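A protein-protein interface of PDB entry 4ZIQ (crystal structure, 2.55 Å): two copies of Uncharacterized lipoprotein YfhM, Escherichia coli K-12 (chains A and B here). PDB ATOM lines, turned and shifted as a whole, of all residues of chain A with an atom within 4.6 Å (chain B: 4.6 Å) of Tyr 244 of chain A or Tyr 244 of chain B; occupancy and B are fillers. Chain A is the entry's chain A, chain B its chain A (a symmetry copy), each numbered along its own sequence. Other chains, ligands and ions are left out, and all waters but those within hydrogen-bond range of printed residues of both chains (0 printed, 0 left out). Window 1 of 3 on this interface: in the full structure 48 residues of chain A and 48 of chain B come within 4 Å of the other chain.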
ATOM      1  N   LEU A 184       0.175   6.642   3.520  1.00  0.00           N
ATOM      2  CA  LEU A 184       0.196   6.328   4.951  1.00  0.00           C
ATOM      3  C   LEU A 184       1.228   5.228   5.300  1.00  0.00           C
ATOM      4  O   LEU A 184       1.154   4.108   4.781  1.00  0.00           O
ATOM      5  CB  LEU A 184      -1.213   5.913   5.425  1.00  0.00           C
ATOM      6  CG  LEU A 184      -1.361   5.497   6.896  1.00  0.00           C
ATOM      7  CD1 LEU A 184      -1.761   6.670   7.769  1.00  0.00           C
ATOM      8  CD2 LEU A 184      -2.375   4.395   7.038  1.00  0.00           C
ATOM      9  N   ALA A 185       2.162   5.558   6.213  1.00  0.00           N
ATOM     10  CA  ALA A 185       3.192   4.646   6.714  1.00  0.00           C
ATOM     11  C   ALA A 185       2.562   3.632   7.670  1.00  0.00           C
ATOM     12  O   ALA A 185       1.681   3.998   8.451  1.00  0.00           O
ATOM     13  CB  ALA A 185       4.289   5.432   7.417  1.00  0.00           C
ATOM     14  N   ASN A 186       2.999   2.364   7.600  1.00  0.00           N
ATOM     15  CA  ASN A 186       2.447   1.268   8.397  1.00  0.00           C
ATOM     16  C   ASN A 186       2.733   1.374   9.911  1.00  0.00           C
ATOM     17  O   ASN A 186       1.875   0.974  10.698  1.00  0.00           O
ATOM     18  CB  ASN A 186       2.931  -0.080   7.869  1.00  0.00           C
ATOM     19  CG  ASN A 186       2.342  -0.462   6.528  1.00  0.00           C
ATOM     20  OD1 ASN A 186       1.147  -0.284   6.254  1.00  0.00           O
ATOM     21  ND2 ASN A 186       3.164  -1.034   5.669  1.00  0.00           N
ATOM     22  N   TRP A 187       3.906   1.891  10.327  1.00  0.00           N
ATOM     23  CA  TRP A 187       4.207   2.011  11.760  1.00  0.00           C
ATOM     24  C   TRP A 187       3.515   3.235  12.372  1.00  0.00           C
ATOM     25  O   TRP A 187       2.947   3.140  13.463  1.00  0.00           O
ATOM     26  CB  TRP A 187       5.719   2.064  12.020  1.00  0.00           C
ATOM     27  CG  TRP A 187       6.210   0.988  12.946  1.00  0.00           C
ATOM     28  CD1 TRP A 187       6.879  -0.146  12.595  1.00  0.00           C
ATOM     29  CD2 TRP A 187       6.057   0.940  14.373  1.00  0.00           C
ATOM     30  NE1 TRP A 187       7.166  -0.895  13.715  1.00  0.00           N
ATOM     31  CE2 TRP A 187       6.672  -0.254  14.821  1.00  0.00           C
ATOM     32  CE3 TRP A 187       5.464   1.793  15.322  1.00  0.00           C
ATOM     33  CZ2 TRP A 187       6.710  -0.616  16.175  1.00  0.00           C
ATOM     34  CZ3 TRP A 187       5.503   1.431  16.664  1.00  0.00           C
ATOM     35  CH2 TRP A 187       6.121   0.242  17.077  1.00  0.00           C
ATOM     36  N   ASP A 243       2.651  -3.431   0.993  1.00  0.00           N
ATOM     37  CA  ASP A 243       3.696  -2.418   0.817  1.00  0.00           C
ATOM     38  C   ASP A 243       3.889  -1.561   2.071  1.00  0.00           C
ATOM     39  O   ASP A 243       2.967  -1.437   2.885  1.00  0.00           O
ATOM     40  CB  ASP A 243       3.357  -1.504  -0.379  1.00  0.00           C
ATOM     41  CG  ASP A 243       3.854  -2.004  -1.721  1.00  0.00           C
ATOM     42  OD1 ASP A 243       3.010  -2.282  -2.599  1.00  0.00           O
ATOM     43  OD2 ASP A 243       5.092  -2.077  -1.909  1.00  0.00           O
ATOM     44  N   TYR A 244       5.091  -0.942   2.194  1.00  0.00           N
ATOM     45  CA  TYR A 244       5.503  -0.046   3.281  1.00  0.00           C
ATOM     46  C   TYR A 244       4.491   1.088   3.491  1.00  0.00           C
ATOM     47  O   TYR A 244       4.140   1.391   4.633  1.00  0.00           O
ATOM     48  CB  TYR A 244       6.888   0.553   2.970  1.00  0.00           C
ATOM     49  CG  TYR A 244       7.903   0.504   4.095  1.00  0.00           C
ATOM     50  CD1 TYR A 244       9.258   0.702   3.845  1.00  0.00           C
ATOM     51  CD2 TYR A 244       7.509   0.286   5.414  1.00  0.00           C
ATOM     52  CE1 TYR A 244      10.199   0.655   4.873  1.00  0.00           C
ATOM     53  CE2 TYR A 244       8.441   0.246   6.451  1.00  0.00           C
ATOM     54  CZ  TYR A 244       9.787   0.427   6.174  1.00  0.00           C
ATOM     55  OH  TYR A 244      10.715   0.389   7.189  1.00  0.00           O
ATOM     56  N   SER A 245       4.022   1.701   2.385  1.00  0.00           N
ATOM     57  CA  SER A 245       3.040   2.783   2.408  1.00  0.00           C
ATOM     58  C   SER A 245       1.939   2.538   1.386  1.00  0.00           C
ATOM     59  O   SER A 245       2.196   1.988   0.310  1.00  0.00           O
ATOM     60  CB  SER A 245       3.707   4.134   2.158  1.00  0.00           C
ATOM     61  OG  SER A 245       4.228   4.238   0.843  1.00  0.00           O
ATOM     62  N   ASN A 246       0.713   2.947   1.735  1.00  0.00           N
ATOM     63  CA  ASN A 246      -0.477   2.818   0.894  1.00  0.00           C
ATOM     64  C   ASN A 246      -1.100   4.203   0.658  1.00  0.00           C
ATOM     65  O   ASN A 246      -1.157   4.990   1.611  1.00  0.00           O
ATOM     66  CB  ASN A 246      -1.492   1.863   1.533  1.00  0.00           C
ATOM     67  CG  ASN A 246      -0.939   0.496   1.850  1.00  0.00           C
ATOM     68  OD1 ASN A 246      -0.640  -0.308   0.958  1.00  0.00           O
ATOM     69  ND2 ASN A 246      -0.797   0.206   3.134  1.00  0.00           N
ATOM     70  N   LEU B 184       4.088 -12.472   7.785  1.00  0.00           N
ATOM     71  CA  LEU B 184       4.672 -11.996   6.528  1.00  0.00           C
ATOM     72  C   LEU B 184       5.087 -10.506   6.597  1.00  0.00           C
ATOM     73  O   LEU B 184       4.253  -9.631   6.854  1.00  0.00           O
ATOM     74  CB  LEU B 184       3.687 -12.225   5.362  1.00  0.00           C
ATOM     75  CG  LEU B 184       4.121 -11.732   3.974  1.00  0.00           C
ATOM     76  CD1 LEU B 184       4.811 -12.827   3.185  1.00  0.00           C
ATOM     77  CD2 LEU B 184       2.938 -11.222   3.197  1.00  0.00           C
ATOM     78  N   ALA B 185       6.380 -10.237   6.327  1.00  0.00           N
ATOM     79  CA  ALA B 185       6.958  -8.892   6.291  1.00  0.00           C
ATOM     80  C   ALA B 185       6.503  -8.170   5.022  1.00  0.00           C
ATOM     81  O   ALA B 185       6.421  -8.795   3.963  1.00  0.00           O
ATOM     82  CB  ALA B 185       8.477  -8.974   6.344  1.00  0.00           C
ATOM     83  N   ASN B 186       6.197  -6.867   5.130  1.00  0.00           N
ATOM     84  CA  ASN B 186       5.682  -6.058   4.024  1.00  0.00           C
ATOM     85  C   ASN B 186       6.698  -5.814   2.886  1.00  0.00           C
ATOM     86  O   ASN B 186       6.278  -5.757   1.730  1.00  0.00           O
ATOM     87  CB  ASN B 186       5.144  -4.725   4.536  1.00  0.00           C
ATOM     88  CG  ASN B 186       3.865  -4.846   5.338  1.00  0.00           C
ATOM     89  OD1 ASN B 186       2.939  -5.594   4.999  1.00  0.00           O
ATOM     90  ND2 ASN B 186       3.770  -4.078   6.407  1.00  0.00           N
ATOM     91  N   TRP B 187       8.003  -5.664   3.186  1.00  0.00           N
ATOM     92  CA  TRP B 187       8.995  -5.436   2.126  1.00  0.00           C
ATOM     93  C   TRP B 187       9.365  -6.746   1.421  1.00  0.00           C
ATOM     94  O   TRP B 187       9.451  -6.781   0.192  1.00  0.00           O
ATOM     95  CB  TRP B 187      10.254  -4.743   2.667  1.00  0.00           C
ATOM     96  CG  TRP B 187      10.574  -3.449   1.976  1.00  0.00           C
ATOM     97  CD1 TRP B 187      10.359  -2.192   2.458  1.00  0.00           C
ATOM     98  CD2 TRP B 187      11.153  -3.286   0.672  1.00  0.00           C
ATOM     99  NE1 TRP B 187      10.779  -1.254   1.542  1.00  0.00           N
ATOM    100  CE2 TRP B 187      11.270  -1.896   0.435  1.00  0.00           C
ATOM    101  CE3 TRP B 187      11.592  -4.180  -0.322  1.00  0.00           C
ATOM    102  CZ2 TRP B 187      11.806  -1.379  -0.752  1.00  0.00           C
ATOM    103  CZ3 TRP B 187      12.122  -3.666  -1.499  1.00  0.00           C
ATOM    104  CH2 TRP B 187      12.226  -2.282  -1.704  1.00  0.00           C
ATOM    105  N   ASP B 243      -0.058  -2.849   9.829  1.00  0.00           N
ATOM    106  CA  ASP B 243       1.088  -3.272  10.638  1.00  0.00           C
ATOM    107  C   ASP B 243       2.256  -3.763   9.777  1.00  0.00           C
ATOM    108  O   ASP B 243       2.047  -4.192   8.636  1.00  0.00           O
ATOM    109  CB  ASP B 243       0.668  -4.390  11.614  1.00  0.00           C
ATOM    110  CG  ASP B 243       0.128  -3.902  12.944  1.00  0.00           C
ATOM    111  OD1 ASP B 243      -1.057  -4.170  13.235  1.00  0.00           O
ATOM    112  OD2 ASP B 243       0.904  -3.287  13.714  1.00  0.00           O
ATOM    113  N   TYR B 244       3.483  -3.729  10.355  1.00  0.00           N
ATOM    114  CA  TYR B 244       4.744  -4.174   9.752  1.00  0.00           C
ATOM    115  C   TYR B 244       4.638  -5.609   9.219  1.00  0.00           C
ATOM    116  O   TYR B 244       5.094  -5.884   8.107  1.00  0.00           O
ATOM    117  CB  TYR B 244       5.880  -4.095  10.791  1.00  0.00           C
ATOM    118  CG  TYR B 244       7.160  -3.428  10.330  1.00  0.00           C
ATOM    119  CD1 TYR B 244       8.116  -3.004  11.247  1.00  0.00           C
ATOM    120  CD2 TYR B 244       7.430  -3.244   8.975  1.00  0.00           C
ATOM    121  CE1 TYR B 244       9.296  -2.386  10.832  1.00  0.00           C
ATOM    122  CE2 TYR B 244       8.610  -2.635   8.548  1.00  0.00           C
ATOM    123  CZ  TYR B 244       9.539  -2.204   9.482  1.00  0.00           C
ATOM    124  OH  TYR B 244      10.707  -1.602   9.073  1.00  0.00           O
ATOM    125  N   SER B 245       4.029  -6.512  10.013  1.00  0.00           N
ATOM    126  CA  SER B 245       3.827  -7.913   9.649  1.00  0.00           C
ATOM    127  C   SER B 245       2.398  -8.348   9.940  1.00  0.00           C
ATOM    128  O   SER B 245       1.792  -7.893  10.915  1.00  0.00           O
ATOM    129  CB  SER B 245       4.818  -8.817  10.378  1.00  0.00           C
ATOM    130  OG  SER B 245       4.589  -8.843  11.777  1.00  0.00           O
ATOM    131  N   ASN B 246       1.867  -9.230   9.083  1.00  0.00           N
ATOM    132  CA  ASN B 246       0.517  -9.785   9.191  1.00  0.00           C
ATOM    133  C   ASN B 246       0.590 -11.319   9.267  1.00  0.00           C
ATOM    134  O   ASN B 246       1.391 -11.905   8.529  1.00  0.00           O
ATOM    135  CB  ASN B 246      -0.348  -9.337   8.008  1.00  0.00           C
ATOM    136  CG  ASN B 246      -0.423  -7.841   7.829  1.00  0.00           C
ATOM    137  OD1 ASN B 246      -1.025  -7.118   8.634  1.00  0.00           O
ATOM    138  ND2 ASN B 246       0.188  -7.347   6.762  1.00  0.00           N
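Printed residues of chain B within 4 Å of Asn 186 of chain A: Asn 186.
Tyr 244 of chain A touches two residues of chain B.
Of the printed residues of chain A, Asn 186 of chain B touches Asn 186.
Printed residues of chain A within 4 Å of Trp 187 of chain B: Tyr 244.
Of chain A, only Trp 187 (3.4 Å) and Tyr 244 (2.7 Å) come within 4 Å of Tyr 244 of chain B.
The nearest residue of chain A that does not touch Tyr 244 of chain B is Asn 186 of chain A (4.4 Å).
The nearest printed residue of chain B that does not touch Trp 187 of chain A is Asp 243 of chain B (5.9 Å).
NE1 of Trp 187 of chain A touches CD1 of Tyr 244 of chain B, at 3.4 Å.
Trp 187 of chain B touches Tyr 244 of chain A (NE1 to CD1, 3.4 Å).
ND2 of Asn 186 of chain A is in hydrogen-bond range of O of Asp 243 of chain A (2.8 Å).
O of Asp 243 of chain B sits at hydrogen-bond distance from ND2 of Asn 186 of chain B (2.8 Å).
ND2 of Asn 186 of chain A lies within hydrogen-bond range of O of Tyr 244 of chain A (2.8 Å).
The backbone carbonyl oxygen of Tyr 244 of chain B sits at hydrogen-bond distance from the side-chain amide nitrogen of Asn 186 of chain B (2.8 Å).
OH of Tyr 244 of chain A lies within hydrogen-bond range of OH of Tyr 244 of chain B (2.7 Å).
ND2 of Asn 186 of chain B sits close to ND2 of Asn 186 of chain A (3.2 Å).
Printed residues of chain A that touch a printed residue of chain B: Asn 186, Trp 187 and Tyr 244.
Hydrophobic or aromatic side chains of chain A within 4 Å of the printed part of chain B: Trp 187 and Tyr 244.
Among the printed residues, 4 pairs touch across the chains.
Among the printed residues, no Asp or Glu carboxylate lies within 4 Å of a Lys or Arg side-chain nitrogen of the other chain.
Asn 186 of chain A touches its own counterpart, Asn 186 of chain B.
Trp 187 of chain A touches Tyr 244 of chain B, and with the chains exchanged Tyr 244 of chain A touches Trp 187 of chain B.
Tyr 244 of chain A touches its own counterpart, Tyr 244 of chain B.
Of the 4 pairs that touch across the chains among the printed residues, 4 have their exchanged pair printed and touching as well.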
